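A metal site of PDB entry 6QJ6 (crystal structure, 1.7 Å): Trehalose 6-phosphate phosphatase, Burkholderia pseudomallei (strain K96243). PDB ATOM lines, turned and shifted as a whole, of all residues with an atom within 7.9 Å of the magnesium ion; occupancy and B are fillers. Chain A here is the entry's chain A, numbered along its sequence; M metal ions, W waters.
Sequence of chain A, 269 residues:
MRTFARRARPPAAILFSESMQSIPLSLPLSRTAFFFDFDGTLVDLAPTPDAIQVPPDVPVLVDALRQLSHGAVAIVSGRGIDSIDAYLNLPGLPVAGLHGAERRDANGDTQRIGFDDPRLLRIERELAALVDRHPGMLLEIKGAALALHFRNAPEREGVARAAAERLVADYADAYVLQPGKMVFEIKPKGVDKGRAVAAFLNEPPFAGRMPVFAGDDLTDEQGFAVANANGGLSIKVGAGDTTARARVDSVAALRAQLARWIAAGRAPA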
ATOM      1  N   ASP A  37     -13.710  24.521 -10.947  1.00  0.00           N
ATOM      2  CA  ASP A  37     -13.958  23.294 -11.698  1.00  0.00           C
ATOM      3  C   ASP A  37     -15.138  23.520 -12.645  1.00  0.00           C
ATOM      4  O   ASP A  37     -15.917  24.465 -12.487  1.00  0.00           O
ATOM      5  CB  ASP A  37     -14.231  22.145 -10.733  1.00  0.00           C
ATOM      6  CG  ASP A  37     -14.564  20.839 -11.436  1.00  0.00           C
ATOM      7  OD1 ASP A  37     -13.756  20.384 -12.286  1.00  0.00           O
ATOM      8  OD2 ASP A  37     -15.627  20.257 -11.117  1.00  0.00           O
ATOM      9  N   PHE A  38     -15.266  22.643 -13.648  1.00  0.00           N
ATOM     10  CA  PHE A  38     -16.319  22.816 -14.640  1.00  0.00           C
ATOM     11  C   PHE A  38     -17.497  21.858 -14.411  1.00  0.00           C
ATOM     12  O   PHE A  38     -18.518  22.271 -13.851  1.00  0.00           O
ATOM     13  CB  PHE A  38     -15.751  22.637 -16.052  1.00  0.00           C
ATOM     14  CG  PHE A  38     -16.614  23.231 -17.128  1.00  0.00           C
ATOM     15  CD1 PHE A  38     -16.905  24.587 -17.135  1.00  0.00           C
ATOM     16  CD2 PHE A  38     -17.141  22.437 -18.133  1.00  0.00           C
ATOM     17  CE1 PHE A  38     -17.707  25.139 -18.135  1.00  0.00           C
ATOM     18  CE2 PHE A  38     -17.940  22.975 -19.131  1.00  0.00           C
ATOM     19  CZ  PHE A  38     -18.231  24.333 -19.128  1.00  0.00           C
ATOM     20  N   ASP A  39     -17.360  20.591 -14.822  1.00  0.00           N
ATOM     21  CA  ASP A  39     -18.457  19.629 -14.686  1.00  0.00           C
ATOM     22  C   ASP A  39     -18.829  19.420 -13.220  1.00  0.00           C
ATOM     23  O   ASP A  39     -17.960  19.178 -12.371  1.00  0.00           O
ATOM     24  CB  ASP A  39     -18.079  18.289 -15.316  1.00  0.00           C
ATOM     25  CG  ASP A  39     -18.040  18.358 -16.827  1.00  0.00           C
ATOM     26  OD1 ASP A  39     -18.924  17.769 -17.470  1.00  0.00           O
ATOM     27  OD2 ASP A  39     -17.114  18.994 -17.374  1.00  0.00           O
ATOM     28  N   GLY A  40     -20.123  19.487 -12.932  1.00  0.00           N
ATOM     29  CA  GLY A  40     -20.610  19.327 -11.573  1.00  0.00           C
ATOM     30  C   GLY A  40     -20.429  20.533 -10.683  1.00  0.00           C
ATOM     31  O   GLY A  40     -20.884  20.509  -9.533  1.00  0.00           O
ATOM     32  N   THR A  41     -19.785  21.591 -11.187  1.00  0.00           N
ATOM     33  CA  THR A  41     -19.510  22.791 -10.411  1.00  0.00           C
ATOM     34  C   THR A  41     -20.144  24.016 -11.054  1.00  0.00           C
ATOM     35  O   THR A  41     -20.973  24.668 -10.423  1.00  0.00           O
ATOM     36  CB  THR A  41     -17.986  22.964 -10.253  1.00  0.00           C
ATOM     37  OG1 THR A  41     -17.482  21.930  -9.408  1.00  0.00           O
ATOM     38  CG2 THR A  41     -17.635  24.300  -9.638  1.00  0.00           C
ATOM     39  N   LEU A  42     -19.776  24.353 -12.289  1.00  0.00           N
ATOM     40  CA  LEU A  42     -20.409  25.430 -13.026  1.00  0.00           C
ATOM     41  C   LEU A  42     -21.524  24.934 -13.922  1.00  0.00           C
ATOM     42  O   LEU A  42     -22.363  25.731 -14.376  1.00  0.00           O
ATOM     43  CB  LEU A  42     -19.390  26.165 -13.911  1.00  0.00           C
ATOM     44  CG  LEU A  42     -18.275  26.898 -13.150  1.00  0.00           C
ATOM     45  CD1 LEU A  42     -17.296  27.513 -14.143  1.00  0.00           C
ATOM     46  CD2 LEU A  42     -18.889  27.952 -12.254  1.00  0.00           C
ATOM     47  N   VAL A  43     -21.536  23.635 -14.180  1.00  0.00           N
ATOM     48  CA  VAL A  43     -22.472  23.022 -15.112  1.00  0.00           C
ATOM     49  C   VAL A  43     -22.854  21.672 -14.523  1.00  0.00           C
ATOM     50  O   VAL A  43     -22.059  21.036 -13.823  1.00  0.00           O
ATOM     51  CB  VAL A  43     -21.844  22.926 -16.521  1.00  0.00           C
ATOM     52  CG1 VAL A  43     -20.877  21.749 -16.632  1.00  0.00           C
ATOM     53  CG2 VAL A  43     -22.887  22.848 -17.579  1.00  0.00           C
ATOM     54  N   LEU A  45     -23.585  17.791 -13.961  1.00  0.00           N
ATOM     55  CA  LEU A  45     -23.024  16.534 -14.450  1.00  0.00           C
ATOM     56  C   LEU A  45     -24.067  15.819 -15.289  1.00  0.00           C
ATOM     57  O   LEU A  45     -25.242  15.736 -14.926  1.00  0.00           O
ATOM     58  CB  LEU A  45     -22.593  15.646 -13.294  1.00  0.00           C
ATOM     59  CG  LEU A  45     -21.103  15.595 -12.940  1.00  0.00           C
ATOM     60  CD1 LEU A  45     -20.929  14.870 -11.621  1.00  0.00           C
ATOM     61  CD2 LEU A  45     -20.304  14.906 -14.031  1.00  0.00           C
ATOM     62  N   VAL A  76     -10.163  25.238 -13.576  1.00  0.00           N
ATOM     63  CA  VAL A  76      -9.264  24.161 -13.154  1.00  0.00           C
ATOM     64  C   VAL A  76     -10.077  22.876 -13.244  1.00  0.00           C
ATOM     65  O   VAL A  76     -10.788  22.503 -12.315  1.00  0.00           O
ATOM     66  CB  VAL A  76      -8.694  24.387 -11.751  1.00  0.00           C
ATOM     67  CG1 VAL A  76      -7.583  23.381 -11.441  1.00  0.00           C
ATOM     68  CG2 VAL A  76      -8.156  25.808 -11.636  1.00  0.00           C
ATOM     69  N   SER A  77      -9.985  22.197 -14.393  1.00  0.00           N
ATOM     70  CA  SER A  77     -10.909  21.119 -14.731  1.00  0.00           C
ATOM     71  C   SER A  77     -10.191  19.790 -14.947  1.00  0.00           C
ATOM     72  O   SER A  77      -8.974  19.717 -15.119  1.00  0.00           O
ATOM     73  CB  SER A  77     -11.720  21.487 -15.981  1.00  0.00           C
ATOM     74  OG  SER A  77     -10.833  21.882 -17.022  1.00  0.00           O
ATOM     75  N   GLY A  78     -10.994  18.719 -14.944  1.00  0.00           N
ATOM     76  CA  GLY A  78     -10.555  17.442 -15.476  1.00  0.00           C
ATOM     77  C   GLY A  78     -10.687  17.312 -16.974  1.00  0.00           C
ATOM     78  O   GLY A  78     -10.105  16.409 -17.570  1.00  0.00           O
ATOM     79  N   HIS A  99      -6.763  17.836 -14.940  1.00  0.00           N
ATOM     80  CA  HIS A  99      -6.356  17.802 -13.544  1.00  0.00           C
ATOM     81  C   HIS A  99      -4.988  18.438 -13.303  1.00  0.00           C
ATOM     82  O   HIS A  99      -4.308  18.125 -12.323  1.00  0.00           O
ATOM     83  CB  HIS A  99      -6.355  16.358 -13.002  1.00  0.00           C
ATOM     84  CG  HIS A  99      -7.652  15.639 -13.199  1.00  0.00           C
ATOM     85  ND1 HIS A  99      -8.673  15.676 -12.264  1.00  0.00           N
ATOM     86  CD2 HIS A  99      -8.107  14.889 -14.225  1.00  0.00           C
ATOM     87  CE1 HIS A  99      -9.700  14.970 -12.708  1.00  0.00           C
ATOM     88  NE2 HIS A  99      -9.380  14.480 -13.890  1.00  0.00           N
ATOM     89  N   LYS A 181     -16.698  10.701  -9.431  1.00  0.00           N
ATOM     90  CA  LYS A 181     -18.058  10.190  -9.471  1.00  0.00           C
ATOM     91  C   LYS A 181     -18.257   9.273 -10.678  1.00  0.00           C
ATOM     92  O   LYS A 181     -18.245   9.731 -11.822  1.00  0.00           O
ATOM     93  CB  LYS A 181     -19.053  11.361  -9.490  1.00  0.00           C
ATOM     94  CG  LYS A 181     -18.997  12.209  -8.215  1.00  0.00           C
ATOM     95  CD  LYS A 181     -19.617  13.584  -8.397  1.00  0.00           C
ATOM     96  CE  LYS A 181     -19.594  14.372  -7.108  1.00  0.00           C
ATOM     97  NZ  LYS A 181     -20.534  15.526  -7.187  1.00  0.00           N
ATOM     98  N   LYS A 193      -4.717  19.427  -9.171  1.00  0.00           N
ATOM     99  CA  LYS A 193      -5.426  20.701  -9.189  1.00  0.00           C
ATOM    100  C   LYS A 193      -4.840  21.679  -8.180  1.00  0.00           C
ATOM    101  O   LYS A 193      -4.803  22.889  -8.436  1.00  0.00           O
ATOM    102  CB  LYS A 193      -6.924  20.484  -8.923  1.00  0.00           C
ATOM    103  CG  LYS A 193      -7.651  19.821 -10.077  1.00  0.00           C
ATOM    104  CD  LYS A 193      -9.160  20.042  -9.993  1.00  0.00           C
ATOM    105  CE  LYS A 193      -9.823  19.701 -11.311  1.00  0.00           C
ATOM    106  NZ  LYS A 193     -11.325  19.857 -11.276  1.00  0.00           N
ATOM    107  N   ALA A 214     -13.890  26.561  -6.078  1.00  0.00           N
ATOM    108  CA  ALA A 214     -15.153  25.822  -6.008  1.00  0.00           C
ATOM    109  C   ALA A 214     -15.019  24.518  -6.789  1.00  0.00           C
ATOM    110  O   ALA A 214     -14.501  24.515  -7.906  1.00  0.00           O
ATOM    111  CB  ALA A 214     -16.306  26.670  -6.552  1.00  0.00           C
ATOM    112  N   GLY A 215     -15.471  23.415  -6.182  1.00  0.00           N
ATOM    113  CA  GLY A 215     -15.400  22.110  -6.828  1.00  0.00           C
ATOM    114  C   GLY A 215     -16.421  21.162  -6.240  1.00  0.00           C
ATOM    115  O   GLY A 215     -17.066  21.452  -5.233  1.00  0.00           O
ATOM    116  N   ASP A 216     -16.557  19.999  -6.885  1.00  0.00           N
ATOM    117  CA  ASP A 216     -17.580  19.038  -6.487  1.00  0.00           C
ATOM    118  C   ASP A 216     -17.079  17.607  -6.270  1.00  0.00           C
ATOM    119  O   ASP A 216     -17.850  16.786  -5.755  1.00  0.00           O
ATOM    120  CB  ASP A 216     -18.697  18.978  -7.546  1.00  0.00           C
ATOM    121  CG  ASP A 216     -18.261  18.245  -8.809  1.00  0.00           C
ATOM    122  OD1 ASP A 216     -17.293  18.703  -9.448  1.00  0.00           O
ATOM    123  OD2 ASP A 216     -18.868  17.209  -9.146  1.00  0.00           O
ATOM    124  N   ASP A 217     -15.844  17.277  -6.639  1.00  0.00           N
ATOM    125  CA  ASP A 217     -15.427  15.884  -6.661  1.00  0.00           C
ATOM    126  C   ASP A 217     -14.093  15.738  -5.928  1.00  0.00           C
ATOM    127  O   ASP A 217     -13.523  16.712  -5.416  1.00  0.00           O
ATOM    128  CB  ASP A 217     -15.327  15.364  -8.105  1.00  0.00           C
ATOM    129  CG  ASP A 217     -15.603  13.876  -8.216  1.00  0.00           C
ATOM    130  OD1 ASP A 217     -15.441  13.148  -7.191  1.00  0.00           O
ATOM    131  OD2 ASP A 217     -15.985  13.423  -9.309  1.00  0.00           O
ATOM    132  N   LEU A 218     -13.594  14.504  -5.869  1.00  0.00           N
ATOM    133  CA  LEU A 218     -12.411  14.194  -5.070  1.00  0.00           C
ATOM    134  C   LEU A 218     -11.193  14.946  -5.588  1.00  0.00           C
ATOM    135  O   LEU A 218     -10.360  15.417  -4.789  1.00  0.00           O
ATOM    136  CB  LEU A 218     -12.149  12.695  -5.066  1.00  0.00           C
ATOM    137  CG  LEU A 218     -10.825  12.283  -4.426  1.00  0.00           C
ATOM    138  CD1 LEU A 218     -10.784  12.729  -2.953  1.00  0.00           C
ATOM    139  CD2 LEU A 218     -10.594  10.790  -4.565  1.00  0.00           C
ATOM    140  N   THR A 219     -11.051  15.082  -6.901  1.00  0.00           N
ATOM    141  CA  THR A 219      -9.924  15.803  -7.471  1.00  0.00           C
ATOM    142  C   THR A 219      -9.856  17.231  -6.944  1.00  0.00           C
ATOM    143  O   THR A 219      -8.769  17.791  -6.802  1.00  0.00           O
ATOM    144  CB  THR A 219     -10.032  15.787  -9.001  1.00  0.00           C
ATOM    145  OG1 THR A 219      -8.899  16.464  -9.584  1.00  0.00           O
ATOM    146  CG2 THR A 219     -11.320  16.458  -9.487  1.00  0.00           C
ATOM    147  N   ASP A 220     -11.002  17.816  -6.615  1.00  0.00           N
ATOM    148  CA  ASP A 220     -11.072  19.212  -6.190  1.00  0.00           C
ATOM    149  C   ASP A 220     -10.599  19.427  -4.760  1.00  0.00           C
ATOM    150  O   ASP A 220     -10.335  20.576  -4.382  1.00  0.00           O
ATOM    151  CB  ASP A 220     -12.498  19.732  -6.378  1.00  0.00           C
ATOM    152  CG  ASP A 220     -12.979  19.574  -7.807  1.00  0.00           C
ATOM    153  OD1 ASP A 220     -12.329  20.123  -8.716  1.00  0.00           O
ATOM    154  OD2 ASP A 220     -14.003  18.884  -8.040  1.00  0.00           O
ATOM    155  N   VAL A 237     -19.429  21.960  -3.819  1.00  0.00           N
ATOM    156  CA  VAL A 237     -20.736  21.950  -4.473  1.00  0.00           C
ATOM    157  C   VAL A 237     -21.352  20.566  -4.276  1.00  0.00           C
ATOM    158  O   VAL A 237     -20.774  19.562  -4.701  1.00  0.00           O
ATOM    159  CB  VAL A 237     -20.627  22.288  -5.964  1.00  0.00           C
ATOM    160  CG1 VAL A 237     -21.998  22.274  -6.625  1.00  0.00           C
ATOM    161  CG2 VAL A 237     -19.949  23.639  -6.157  1.00  0.00           C
HETATM  162 MG    MG M   1     -16.370  18.330 -11.243  1.00  0.00          MG
HETATM  163  O   HOH W   1     -17.414  16.448 -11.254  1.00  0.00           O
HETATM  164  O   HOH W   2     -15.401  17.748 -13.021  1.00  0.00           O
HETATM  165  O   HOH W   3     -14.737  17.626 -10.356  1.00  0.00           O
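N of Asp 216 is in hydrogen-bond range of OD2 of Asp 220, 3.0 Å away.
The backbone NH of Asp 216 is in hydrogen-bond range of the side-chain hydroxyl of Thr 41 (3.3 Å).
The backbone NH (N) of Asp 37 is in hydrogen-bond range of the backbone carbonyl oxygen (O) of Ala 214 (3.1 Å).
The side-chain carboxylate (OD2) of Asp 216 lies within salt-bridge range of the side-chain amino group (NZ) of Lys 181.
OD1 of Asp 37 lies within salt-bridge range of NZ of Lys 193 (2.7 Å).
OD2 of Asp 37 sits close to OG1 of Thr 41 (3.0 Å).
The magnesium ion is bound by water W3, the side-chain carboxylate of Asp 216, the side-chain carboxylate of Asp 37, water W2, the backbone carbonyl oxygen of Asp 39 and water W1.
The magnesium ion has six donor atoms within binding distance.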
